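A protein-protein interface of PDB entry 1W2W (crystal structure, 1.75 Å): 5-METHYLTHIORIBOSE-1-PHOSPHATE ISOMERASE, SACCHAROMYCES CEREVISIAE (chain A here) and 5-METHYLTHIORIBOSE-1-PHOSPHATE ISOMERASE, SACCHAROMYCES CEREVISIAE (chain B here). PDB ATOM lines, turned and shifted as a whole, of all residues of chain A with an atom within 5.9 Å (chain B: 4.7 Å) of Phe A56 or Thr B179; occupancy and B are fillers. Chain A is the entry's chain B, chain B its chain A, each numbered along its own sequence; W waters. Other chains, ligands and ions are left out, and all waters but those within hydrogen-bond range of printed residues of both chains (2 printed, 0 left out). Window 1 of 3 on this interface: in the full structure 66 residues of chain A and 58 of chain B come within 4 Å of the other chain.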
ATOM      1  N   VAL A   7     -24.859  25.359  33.581  1.00  0.00           N
ATOM      2  CA  VAL A   7     -24.746  24.135  32.789  1.00  0.00           C
ATOM      3  C   VAL A   7     -24.641  22.929  33.709  1.00  0.00           C
ATOM      4  O   VAL A   7     -23.919  22.991  34.713  1.00  0.00           O
ATOM      5  CB  VAL A   7     -23.465  24.172  31.943  1.00  0.00           C
ATOM      6  CG1 VAL A   7     -23.356  22.887  31.100  1.00  0.00           C
ATOM      7  CG2 VAL A   7     -23.429  25.440  31.089  1.00  0.00           C
ATOM      8  N   PHE A   8     -25.343  21.845  33.361  1.00  0.00           N
ATOM      9  CA  PHE A   8     -25.281  20.588  34.108  1.00  0.00           C
ATOM     10  C   PHE A   8     -24.720  19.507  33.186  1.00  0.00           C
ATOM     11  O   PHE A   8     -25.481  18.812  32.511  1.00  0.00           O
ATOM     12  CB  PHE A   8     -26.705  20.176  34.532  1.00  0.00           C
ATOM     13  CG  PHE A   8     -27.322  21.098  35.552  1.00  0.00           C
ATOM     14  CD1 PHE A   8     -28.536  21.736  35.301  1.00  0.00           C
ATOM     15  CD2 PHE A   8     -26.682  21.316  36.762  1.00  0.00           C
ATOM     16  CE1 PHE A   8     -29.095  22.584  36.252  1.00  0.00           C
ATOM     17  CE2 PHE A   8     -27.237  22.164  37.721  1.00  0.00           C
ATOM     18  CZ  PHE A   8     -28.433  22.801  37.462  1.00  0.00           C
ATOM     19  N   PRO A   9     -23.402  19.363  33.134  1.00  0.00           N
ATOM     20  CA  PRO A   9     -22.817  18.260  32.367  1.00  0.00           C
ATOM     21  C   PRO A   9     -22.981  16.943  33.140  1.00  0.00           C
ATOM     22  O   PRO A   9     -22.892  16.930  34.371  1.00  0.00           O
ATOM     23  CB  PRO A   9     -21.337  18.639  32.285  1.00  0.00           C
ATOM     24  CG  PRO A   9     -21.104  19.434  33.537  1.00  0.00           C
ATOM     25  CD  PRO A   9     -22.381  20.216  33.775  1.00  0.00           C
ATOM     26  N   LEU A  10     -23.205  15.859  32.406  1.00  0.00           N
ATOM     27  CA  LEU A  10     -23.257  14.527  32.984  1.00  0.00           C
ATOM     28  C   LEU A  10     -21.859  13.930  33.072  1.00  0.00           C
ATOM     29  O   LEU A  10     -21.044  14.139  32.167  1.00  0.00           O
ATOM     30  CB  LEU A  10     -24.138  13.641  32.105  1.00  0.00           C
ATOM     31  CG  LEU A  10     -25.549  14.113  31.754  1.00  0.00           C
ATOM     32  CD1 LEU A  10     -26.271  12.925  31.104  1.00  0.00           C
ATOM     33  CD2 LEU A  10     -26.287  14.581  32.987  1.00  0.00           C
ATOM     34  N   THR A  12     -20.817  10.937  32.471  1.00  0.00           N
ATOM     35  CA  THR A  12     -20.587  10.166  31.243  1.00  0.00           C
ATOM     36  C   THR A  12     -19.658   8.975  31.464  1.00  0.00           C
ATOM     37  O   THR A  12     -18.551   8.892  30.917  1.00  0.00           O
ATOM     38  CB  THR A  12     -20.088  11.045  30.070  1.00  0.00           C
ATOM     39  OG1 THR A  12     -20.886  12.230  29.984  1.00  0.00           O
ATOM     40  CG2 THR A  12     -20.361  10.328  28.735  1.00  0.00           C
ATOM     41  N   THR A  22     -15.133  17.568  30.040  1.00  0.00           N
ATOM     42  CA  THR A  22     -16.077  18.687  29.942  1.00  0.00           C
ATOM     43  C   THR A  22     -16.024  19.587  31.191  1.00  0.00           C
ATOM     44  O   THR A  22     -16.017  20.819  31.096  1.00  0.00           O
ATOM     45  CB  THR A  22     -17.482  18.140  29.699  1.00  0.00           C
ATOM     46  OG1 THR A  22     -17.552  17.621  28.367  1.00  0.00           O
ATOM     47  CG2 THR A  22     -18.538  19.260  29.751  1.00  0.00           C
ATOM     48  N   LEU A  26     -15.201  23.611  31.237  1.00  0.00           N
ATOM     49  CA  LEU A  26     -16.132  24.577  31.817  1.00  0.00           C
ATOM     50  C   LEU A  26     -15.428  25.404  32.895  1.00  0.00           C
ATOM     51  O   LEU A  26     -15.643  26.618  33.014  1.00  0.00           O
ATOM     52  CB  LEU A  26     -17.360  23.859  32.406  1.00  0.00           C
ATOM     53  CG  LEU A  26     -18.289  23.272  31.336  1.00  0.00           C
ATOM     54  CD1 LEU A  26     -19.283  22.254  31.941  1.00  0.00           C
ATOM     55  CD2 LEU A  26     -19.018  24.394  30.620  1.00  0.00           C
ATOM     56  N   ALA A  54     -33.066  23.124  27.806  1.00  0.00           N
ATOM     57  CA  ALA A  54     -32.556  22.381  26.663  1.00  0.00           C
ATOM     58  C   ALA A  54     -31.485  21.389  27.085  1.00  0.00           C
ATOM     59  O   ALA A  54     -30.776  21.598  28.075  1.00  0.00           O
ATOM     60  CB  ALA A  54     -32.016  23.321  25.584  1.00  0.00           C
ATOM     61  N   ALA A  55     -31.370  20.314  26.315  1.00  0.00           N
ATOM     62  CA  ALA A  55     -30.166  19.486  26.324  1.00  0.00           C
ATOM     63  C   ALA A  55     -29.484  19.663  24.972  1.00  0.00           C
ATOM     64  O   ALA A  55     -30.151  19.659  23.935  1.00  0.00           O
ATOM     65  CB  ALA A  55     -30.527  18.034  26.545  1.00  0.00           C
ATOM     66  N   PHE A  56     -28.166  19.846  24.996  1.00  0.00           N
ATOM     67  CA  PHE A  56     -27.380  19.836  23.776  1.00  0.00           C
ATOM     68  C   PHE A  56     -26.404  18.668  23.827  1.00  0.00           C
ATOM     69  O   PHE A  56     -25.670  18.529  24.792  1.00  0.00           O
ATOM     70  CB  PHE A  56     -26.606  21.149  23.647  1.00  0.00           C
ATOM     71  CG  PHE A  56     -27.487  22.324  23.401  1.00  0.00           C
ATOM     72  CD1 PHE A  56     -28.069  22.513  22.147  1.00  0.00           C
ATOM     73  CD2 PHE A  56     -27.764  23.221  24.421  1.00  0.00           C
ATOM     74  CE1 PHE A  56     -28.895  23.596  21.894  1.00  0.00           C
ATOM     75  CE2 PHE A  56     -28.596  24.315  24.185  1.00  0.00           C
ATOM     76  CZ  PHE A  56     -29.168  24.502  22.920  1.00  0.00           C
ATOM     77  N   VAL A  57     -26.422  17.845  22.782  1.00  0.00           N
ATOM     78  CA  VAL A  57     -25.545  16.686  22.672  1.00  0.00           C
ATOM     79  C   VAL A  57     -24.828  16.774  21.328  1.00  0.00           C
ATOM     80  O   VAL A  57     -25.299  17.428  20.397  1.00  0.00           O
ATOM     81  CB  VAL A  57     -26.316  15.338  22.813  1.00  0.00           C
ATOM     82  CG1 VAL A  57     -27.191  15.367  24.060  1.00  0.00           C
ATOM     83  CG2 VAL A  57     -27.175  15.003  21.563  1.00  0.00           C
ATOM     84  N   GLY A  58     -23.683  16.119  21.236  1.00  0.00           N
ATOM     85  CA  GLY A  58     -22.990  16.033  19.965  1.00  0.00           C
ATOM     86  C   GLY A  58     -23.464  14.825  19.187  1.00  0.00           C
ATOM     87  O   GLY A  58     -24.543  14.283  19.427  1.00  0.00           O
ATOM     88  N   LEU A  77     -30.869  10.172  27.741  1.00  0.00           N
ATOM     89  CA  LEU A  77     -31.102  11.586  27.987  1.00  0.00           C
ATOM     90  C   LEU A  77     -32.276  12.084  27.134  1.00  0.00           C
ATOM     91  O   LEU A  77     -33.091  12.877  27.601  1.00  0.00           O
ATOM     92  CB  LEU A  77     -29.811  12.372  27.694  1.00  0.00           C
ATOM     93  CG  LEU A  77     -29.915  13.905  27.743  1.00  0.00           C
ATOM     94  CD1 LEU A  77     -30.343  14.376  29.136  1.00  0.00           C
ATOM     95  CD2 LEU A  77     -28.560  14.520  27.392  1.00  0.00           C
ATOM     96  N   LYS A  87     -36.592  20.486  25.354  1.00  0.00           N
ATOM     97  CA  LYS A  87     -36.099  20.367  23.984  1.00  0.00           C
ATOM     98  C   LYS A  87     -34.749  19.654  23.952  1.00  0.00           C
ATOM     99  O   LYS A  87     -33.880  19.933  24.771  1.00  0.00           O
ATOM    100  CB  LYS A  87     -35.965  21.748  23.346  1.00  0.00           C
ATOM    101  CG  LYS A  87     -37.302  22.430  23.098  1.00  0.00           C
ATOM    102  CD  LYS A  87     -37.938  21.941  21.819  1.00  0.00           C
ATOM    103  CE  LYS A  87     -39.081  22.863  21.378  1.00  0.00           C
ATOM    104  NZ  LYS A  87     -40.036  23.059  22.504  1.00  0.00           N
ATOM    105  N   PHE A  89     -31.524  18.688  21.468  1.00  0.00           N
ATOM    106  CA  PHE A  89     -30.859  19.041  20.214  1.00  0.00           C
ATOM    107  C   PHE A  89     -29.547  18.295  20.021  1.00  0.00           C
ATOM    108  O   PHE A  89     -28.728  18.214  20.927  1.00  0.00           O
ATOM    109  CB  PHE A  89     -30.558  20.534  20.201  1.00  0.00           C
ATOM    110  CG  PHE A  89     -31.778  21.403  20.293  1.00  0.00           C
ATOM    111  CD1 PHE A  89     -32.645  21.512  19.215  1.00  0.00           C
ATOM    112  CD2 PHE A  89     -32.034  22.135  21.445  1.00  0.00           C
ATOM    113  CE1 PHE A  89     -33.769  22.323  19.294  1.00  0.00           C
ATOM    114  CE2 PHE A  89     -33.147  22.947  21.528  1.00  0.00           C
ATOM    115  CZ  PHE A  89     -34.010  23.040  20.451  1.00  0.00           C
ATOM    116  N   VAL A  90     -29.362  17.761  18.817  1.00  0.00           N
ATOM    117  CA  VAL A  90     -28.092  17.204  18.379  1.00  0.00           C
ATOM    118  C   VAL A  90     -27.331  18.277  17.594  1.00  0.00           C
ATOM    119  O   VAL A  90     -27.907  18.961  16.748  1.00  0.00           O
ATOM    120  CB  VAL A  90     -28.356  15.984  17.479  1.00  0.00           C
ATOM    121  CG1 VAL A  90     -27.079  15.497  16.820  1.00  0.00           C
ATOM    122  CG2 VAL A  90     -29.002  14.861  18.302  1.00  0.00           C
ATOM    123  N   VAL A  91     -26.042  18.427  17.883  1.00  0.00           N
ATOM    124  CA  VAL A  91     -25.248  19.506  17.314  1.00  0.00           C
ATOM    125  C   VAL A  91     -24.035  18.862  16.653  1.00  0.00           C
ATOM    126  O   VAL A  91     -23.243  18.216  17.338  1.00  0.00           O
ATOM    127  CB  VAL A  91     -24.730  20.434  18.443  1.00  0.00           C
ATOM    128  CG1 VAL A  91     -24.020  21.658  17.865  1.00  0.00           C
ATOM    129  CG2 VAL A  91     -25.874  20.870  19.371  1.00  0.00           C
ATOM    130  N   ILE A 171     -28.538  20.778  14.838  1.00  0.00           N
ATOM    131  CA  ILE A 171     -27.926  22.096  14.706  1.00  0.00           C
ATOM    132  C   ILE A 171     -26.575  21.956  14.025  1.00  0.00           C
ATOM    133  O   ILE A 171     -25.708  21.231  14.524  1.00  0.00           O
ATOM    134  CB  ILE A 171     -27.732  22.737  16.096  1.00  0.00           C
ATOM    135  CG1 ILE A 171     -29.099  22.949  16.765  1.00  0.00           C
ATOM    136  CG2 ILE A 171     -26.957  24.051  15.953  1.00  0.00           C
ATOM    137  CD1 ILE A 171     -29.005  23.442  18.215  1.00  0.00           C
ATOM    138  N   GLY B 158     -27.062  27.603  17.030  1.00  0.00           N
ATOM    139  CA  GLY B 158     -27.784  26.941  18.097  1.00  0.00           C
ATOM    140  C   GLY B 158     -28.172  27.896  19.215  1.00  0.00           C
ATOM    141  O   GLY B 158     -29.287  27.822  19.715  1.00  0.00           O
ATOM    142  N   LEU B 162     -32.175  28.672  20.199  1.00  0.00           N
ATOM    143  CA  LEU B 162     -32.790  28.476  21.510  1.00  0.00           C
ATOM    144  C   LEU B 162     -33.334  29.785  22.092  1.00  0.00           C
ATOM    145  O   LEU B 162     -34.459  29.818  22.608  1.00  0.00           O
ATOM    146  CB  LEU B 162     -31.836  27.791  22.498  1.00  0.00           C
ATOM    147  CG  LEU B 162     -32.405  27.525  23.898  1.00  0.00           C
ATOM    148  CD1 LEU B 162     -33.589  26.567  23.829  1.00  0.00           C
ATOM    149  CD2 LEU B 162     -31.297  26.946  24.810  1.00  0.00           C
ATOM    150  N   VAL B 177     -28.931  24.364  31.017  1.00  0.00           N
ATOM    151  CA  VAL B 177     -28.944  23.311  30.001  1.00  0.00           C
ATOM    152  C   VAL B 177     -28.215  22.075  30.509  1.00  0.00           C
ATOM    153  O   VAL B 177     -27.374  22.153  31.428  1.00  0.00           O
ATOM    154  CB  VAL B 177     -28.230  23.766  28.713  1.00  0.00           C
ATOM    155  CG1 VAL B 177     -28.858  25.060  28.169  1.00  0.00           C
ATOM    156  CG2 VAL B 177     -26.741  23.944  29.002  1.00  0.00           C
ATOM    157  N   LEU B 178     -28.571  20.945  29.902  1.00  0.00           N
ATOM    158  CA  LEU B 178     -27.921  19.656  30.141  1.00  0.00           C
ATOM    159  C   LEU B 178     -26.983  19.379  28.976  1.00  0.00           C
ATOM    160  O   LEU B 178     -27.272  19.778  27.846  1.00  0.00           O
ATOM    161  CB  LEU B 178     -28.985  18.555  30.181  1.00  0.00           C
ATOM    162  CG  LEU B 178     -29.788  18.524  31.488  1.00  0.00           C
ATOM    163  CD1 LEU B 178     -31.148  17.858  31.264  1.00  0.00           C
ATOM    164  CD2 LEU B 178     -29.000  17.792  32.586  1.00  0.00           C
ATOM    165  N   THR B 179     -25.874  18.690  29.236  1.00  0.00           N
ATOM    166  CA  THR B 179     -25.076  18.157  28.129  1.00  0.00           C
ATOM    167  C   THR B 179     -24.426  16.823  28.522  1.00  0.00           C
ATOM    168  O   THR B 179     -24.427  16.460  29.686  1.00  0.00           O
ATOM    169  CB  THR B 179     -24.052  19.215  27.625  1.00  0.00           C
ATOM    170  OG1 THR B 179     -23.520  18.819  26.341  1.00  0.00           O
ATOM    171  CG2 THR B 179     -22.828  19.354  28.554  1.00  0.00           C
ATOM    172  N   ILE B 180     -23.890  16.096  27.544  1.00  0.00           N
ATOM    173  CA  ILE B 180     -23.338  14.763  27.791  1.00  0.00           C
ATOM    174  C   ILE B 180     -22.020  14.662  27.035  1.00  0.00           C
ATOM    175  O   ILE B 180     -21.823  15.339  26.016  1.00  0.00           O
ATOM    176  CB  ILE B 180     -24.324  13.665  27.288  1.00  0.00           C
ATOM    177  CG1 ILE B 180     -23.917  12.260  27.771  1.00  0.00           C
ATOM    178  CG2 ILE B 180     -24.470  13.720  25.759  1.00  0.00           C
ATOM    179  CD1 ILE B 180     -24.970  11.169  27.439  1.00  0.00           C
ATOM    180  N   CYS B 181     -21.128  13.821  27.548  1.00  0.00           N
ATOM    181  CA  CYS B 181     -19.857  13.511  26.893  1.00  0.00           C
ATOM    182  C   CYS B 181     -18.958  14.747  26.869  1.00  0.00           C
ATOM    183  O   CYS B 181     -19.089  15.640  27.720  1.00  0.00           O
ATOM    184  CB  CYS B 181     -20.061  12.961  25.475  1.00  0.00           C
ATOM    185  SG  CYS B 181     -18.692  11.898  24.907  1.00  0.00           S
ATOM    186  N   ALA B 194     -21.681  20.724  20.571  1.00  0.00           N
ATOM    187  CA  ALA B 194     -22.653  21.048  21.620  1.00  0.00           C
ATOM    188  C   ALA B 194     -22.051  22.034  22.634  1.00  0.00           C
ATOM    189  O   ALA B 194     -22.720  22.973  23.057  1.00  0.00           O
ATOM    190  CB  ALA B 194     -23.189  19.784  22.311  1.00  0.00           C
ATOM    191  N   VAL B 197     -22.206  25.559  21.304  1.00  0.00           N
ATOM    192  CA  VAL B 197     -23.485  26.229  21.514  1.00  0.00           C
ATOM    193  C   VAL B 197     -23.547  26.787  22.922  1.00  0.00           C
ATOM    194  O   VAL B 197     -24.011  27.903  23.143  1.00  0.00           O
ATOM    195  CB  VAL B 197     -24.669  25.262  21.307  1.00  0.00           C
ATOM    196  CG1 VAL B 197     -25.994  25.946  21.708  1.00  0.00           C
ATOM    197  CG2 VAL B 197     -24.718  24.816  19.844  1.00  0.00           C
ATOM    198  N   ILE B 198     -23.093  25.990  23.884  1.00  0.00           N
ATOM    199  CA  ILE B 198     -23.067  26.429  25.274  1.00  0.00           C
ATOM    200  C   ILE B 198     -22.134  27.637  25.437  1.00  0.00           C
ATOM    201  O   ILE B 198     -22.464  28.610  26.139  1.00  0.00           O
ATOM    202  CB  ILE B 198     -22.693  25.228  26.167  1.00  0.00           C
ATOM    203  CG1 ILE B 198     -23.913  24.299  26.289  1.00  0.00           C
ATOM    204  CG2 ILE B 198     -22.184  25.676  27.544  1.00  0.00           C
ATOM    205  CD1 ILE B 198     -23.517  22.870  26.690  1.00  0.00           C
ATOM    206  N   LEU B 201     -23.976  30.610  24.011  1.00  0.00           N
ATOM    207  CA  LEU B 201     -24.973  31.012  24.997  1.00  0.00           C
ATOM    208  C   LEU B 201     -24.341  31.771  26.166  1.00  0.00           C
ATOM    209  O   LEU B 201     -24.908  32.746  26.678  1.00  0.00           O
ATOM    210  CB  LEU B 201     -25.766  29.795  25.477  1.00  0.00           C
ATOM    211  CG  LEU B 201     -26.827  29.272  24.496  1.00  0.00           C
ATOM    212  CD1 LEU B 201     -27.376  27.934  25.003  1.00  0.00           C
ATOM    213  CD2 LEU B 201     -27.980  30.288  24.337  1.00  0.00           C
HETATM  214  O   HOH W   1     -20.941  16.151  29.928  1.00  0.00           O
HETATM  215  O   HOH W   2     -22.351  14.587  23.251  1.00  0.00           O
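The backbone NH of Phe A8 lies within hydrogen-bond range of the backbone carbonyl oxygen of Val B177 (2.8 Å).
O of Ala A54 sits at hydrogen-bond distance from N of Leu B178 (2.9 Å).
The backbone NH (N) of Phe A56 lies within hydrogen-bond range of the backbone carbonyl oxygen (O) of Leu B178, at 3.0 Å.
The backbone NH of Thr B179 lies within hydrogen-bond range of the backbone carbonyl oxygen of Phe A8.
O of Thr B179 sits at hydrogen-bond distance from N of Leu A10.
The side-chain hydroxyl (OG1) of Thr B179 is in hydrogen-bond range of the backbone carbonyl oxygen (O) of Phe A56 (2.7 Å).
The backbone NH of Cys B181 sits at hydrogen-bond distance from the side-chain hydroxyl of Thr A12 (2.9 Å).
O of Cys B181 lies within hydrogen-bond range of OG1 of Thr A22 (2.6 Å).
The side-chain hydroxyl of Thr A12 sits at hydrogen-bond distance from the backbone carbonyl oxygen of Leu A10, at 2.9 Å.
The backbone NH (N) of Ala A55 lies within hydrogen-bond range of the backbone carbonyl oxygen (O) of Lys A87, at 3.0 Å.
O of Ala A55 lies within hydrogen-bond range of N of Phe A89 (3.0 Å).
The backbone NH (N) of Val A57 is in hydrogen-bond range of the backbone carbonyl oxygen (O) of Phe A89 (3.0 Å).
The backbone carbonyl oxygen (O) of Val A57 lies within hydrogen-bond range of the backbone NH (N) of Val A91, at 2.8 Å.
The backbone carbonyl oxygen of Val A90 is in hydrogen-bond range of the backbone NH of Ile A171, 2.7 Å away.
CA of Val A7 touches O of Val B177 (3.6 Å).
Leu B178 touches Phe A8.
Ile B180 touches Thr A12.
Ala A54 touches Leu B162 (CB to CD2, 3.8 Å).
Leu B178 touches Ala A55.
C of Phe A56 touches CB of Ala B194 (3.7 Å).
CZ of Phe A56 touches CG1 of Val B197 (3.7 Å).
Phe A56 touches Leu B201.
CG1 of Val A57 touches CG2 of Ile B180 (3.6 Å).
Ala B194 touches Val A91 (N to CG1, 3.7 Å).
Of the printed residues of chain B, Phe A8 touches Val B177 (2.8 Å), Leu B178 (3.5 Å) and Thr B179 (3.3 Å).
Of the printed residues of chain B, Val A91 touches Ala B194 (3.7 Å) and Val B197 (3.8 Å).
Of chain A, only Phe A8 (3.3 Å), Pro A9 (3.6 Å), Leu A10 (3.0 Å) and Phe A56 (2.7 Å) come within 4 Å of Thr B179.
Of the printed residues of chain A, Ile B180 touches Thr A12 (3.8 Å) and Val A57 (3.6 Å).
Printed residues of chain A within 4 Å of Val B197: Phe A56 (3.7 Å) and Val A91 (3.8 Å).
The nearest residue of chain A that does not touch Thr B179 is Val A7 (4.4 Å).
Printed residues of chain A that touch a printed residue of chain B: Val A7, Phe A8, Pro A9, Leu A10, Thr A12, Thr A22, Ala A54, Ala A55, Phe A56, Val A57, Gly A58, Val A91 and Ile A171.
Hydrophobic or aromatic side chains of chain A within 4 Å of the printed part of chain B: Val A7, Phe A8, Leu A10, Ala A54, Ala A55, Phe A56, Val A57, Val A91 and Ile A171.
Among the printed residues, no Asp or Glu carboxylate lies within 4 Å of a Lys or Arg side-chain nitrogen of the other chain.
Water W2 lies within hydrogen-bond range of N of Gly A58 and O of Ile B180.
Water W1 lies within hydrogen-bond range of the backbone carbonyl oxygen of Cys B181 and the backbone carbonyl oxygen of Leu A10.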
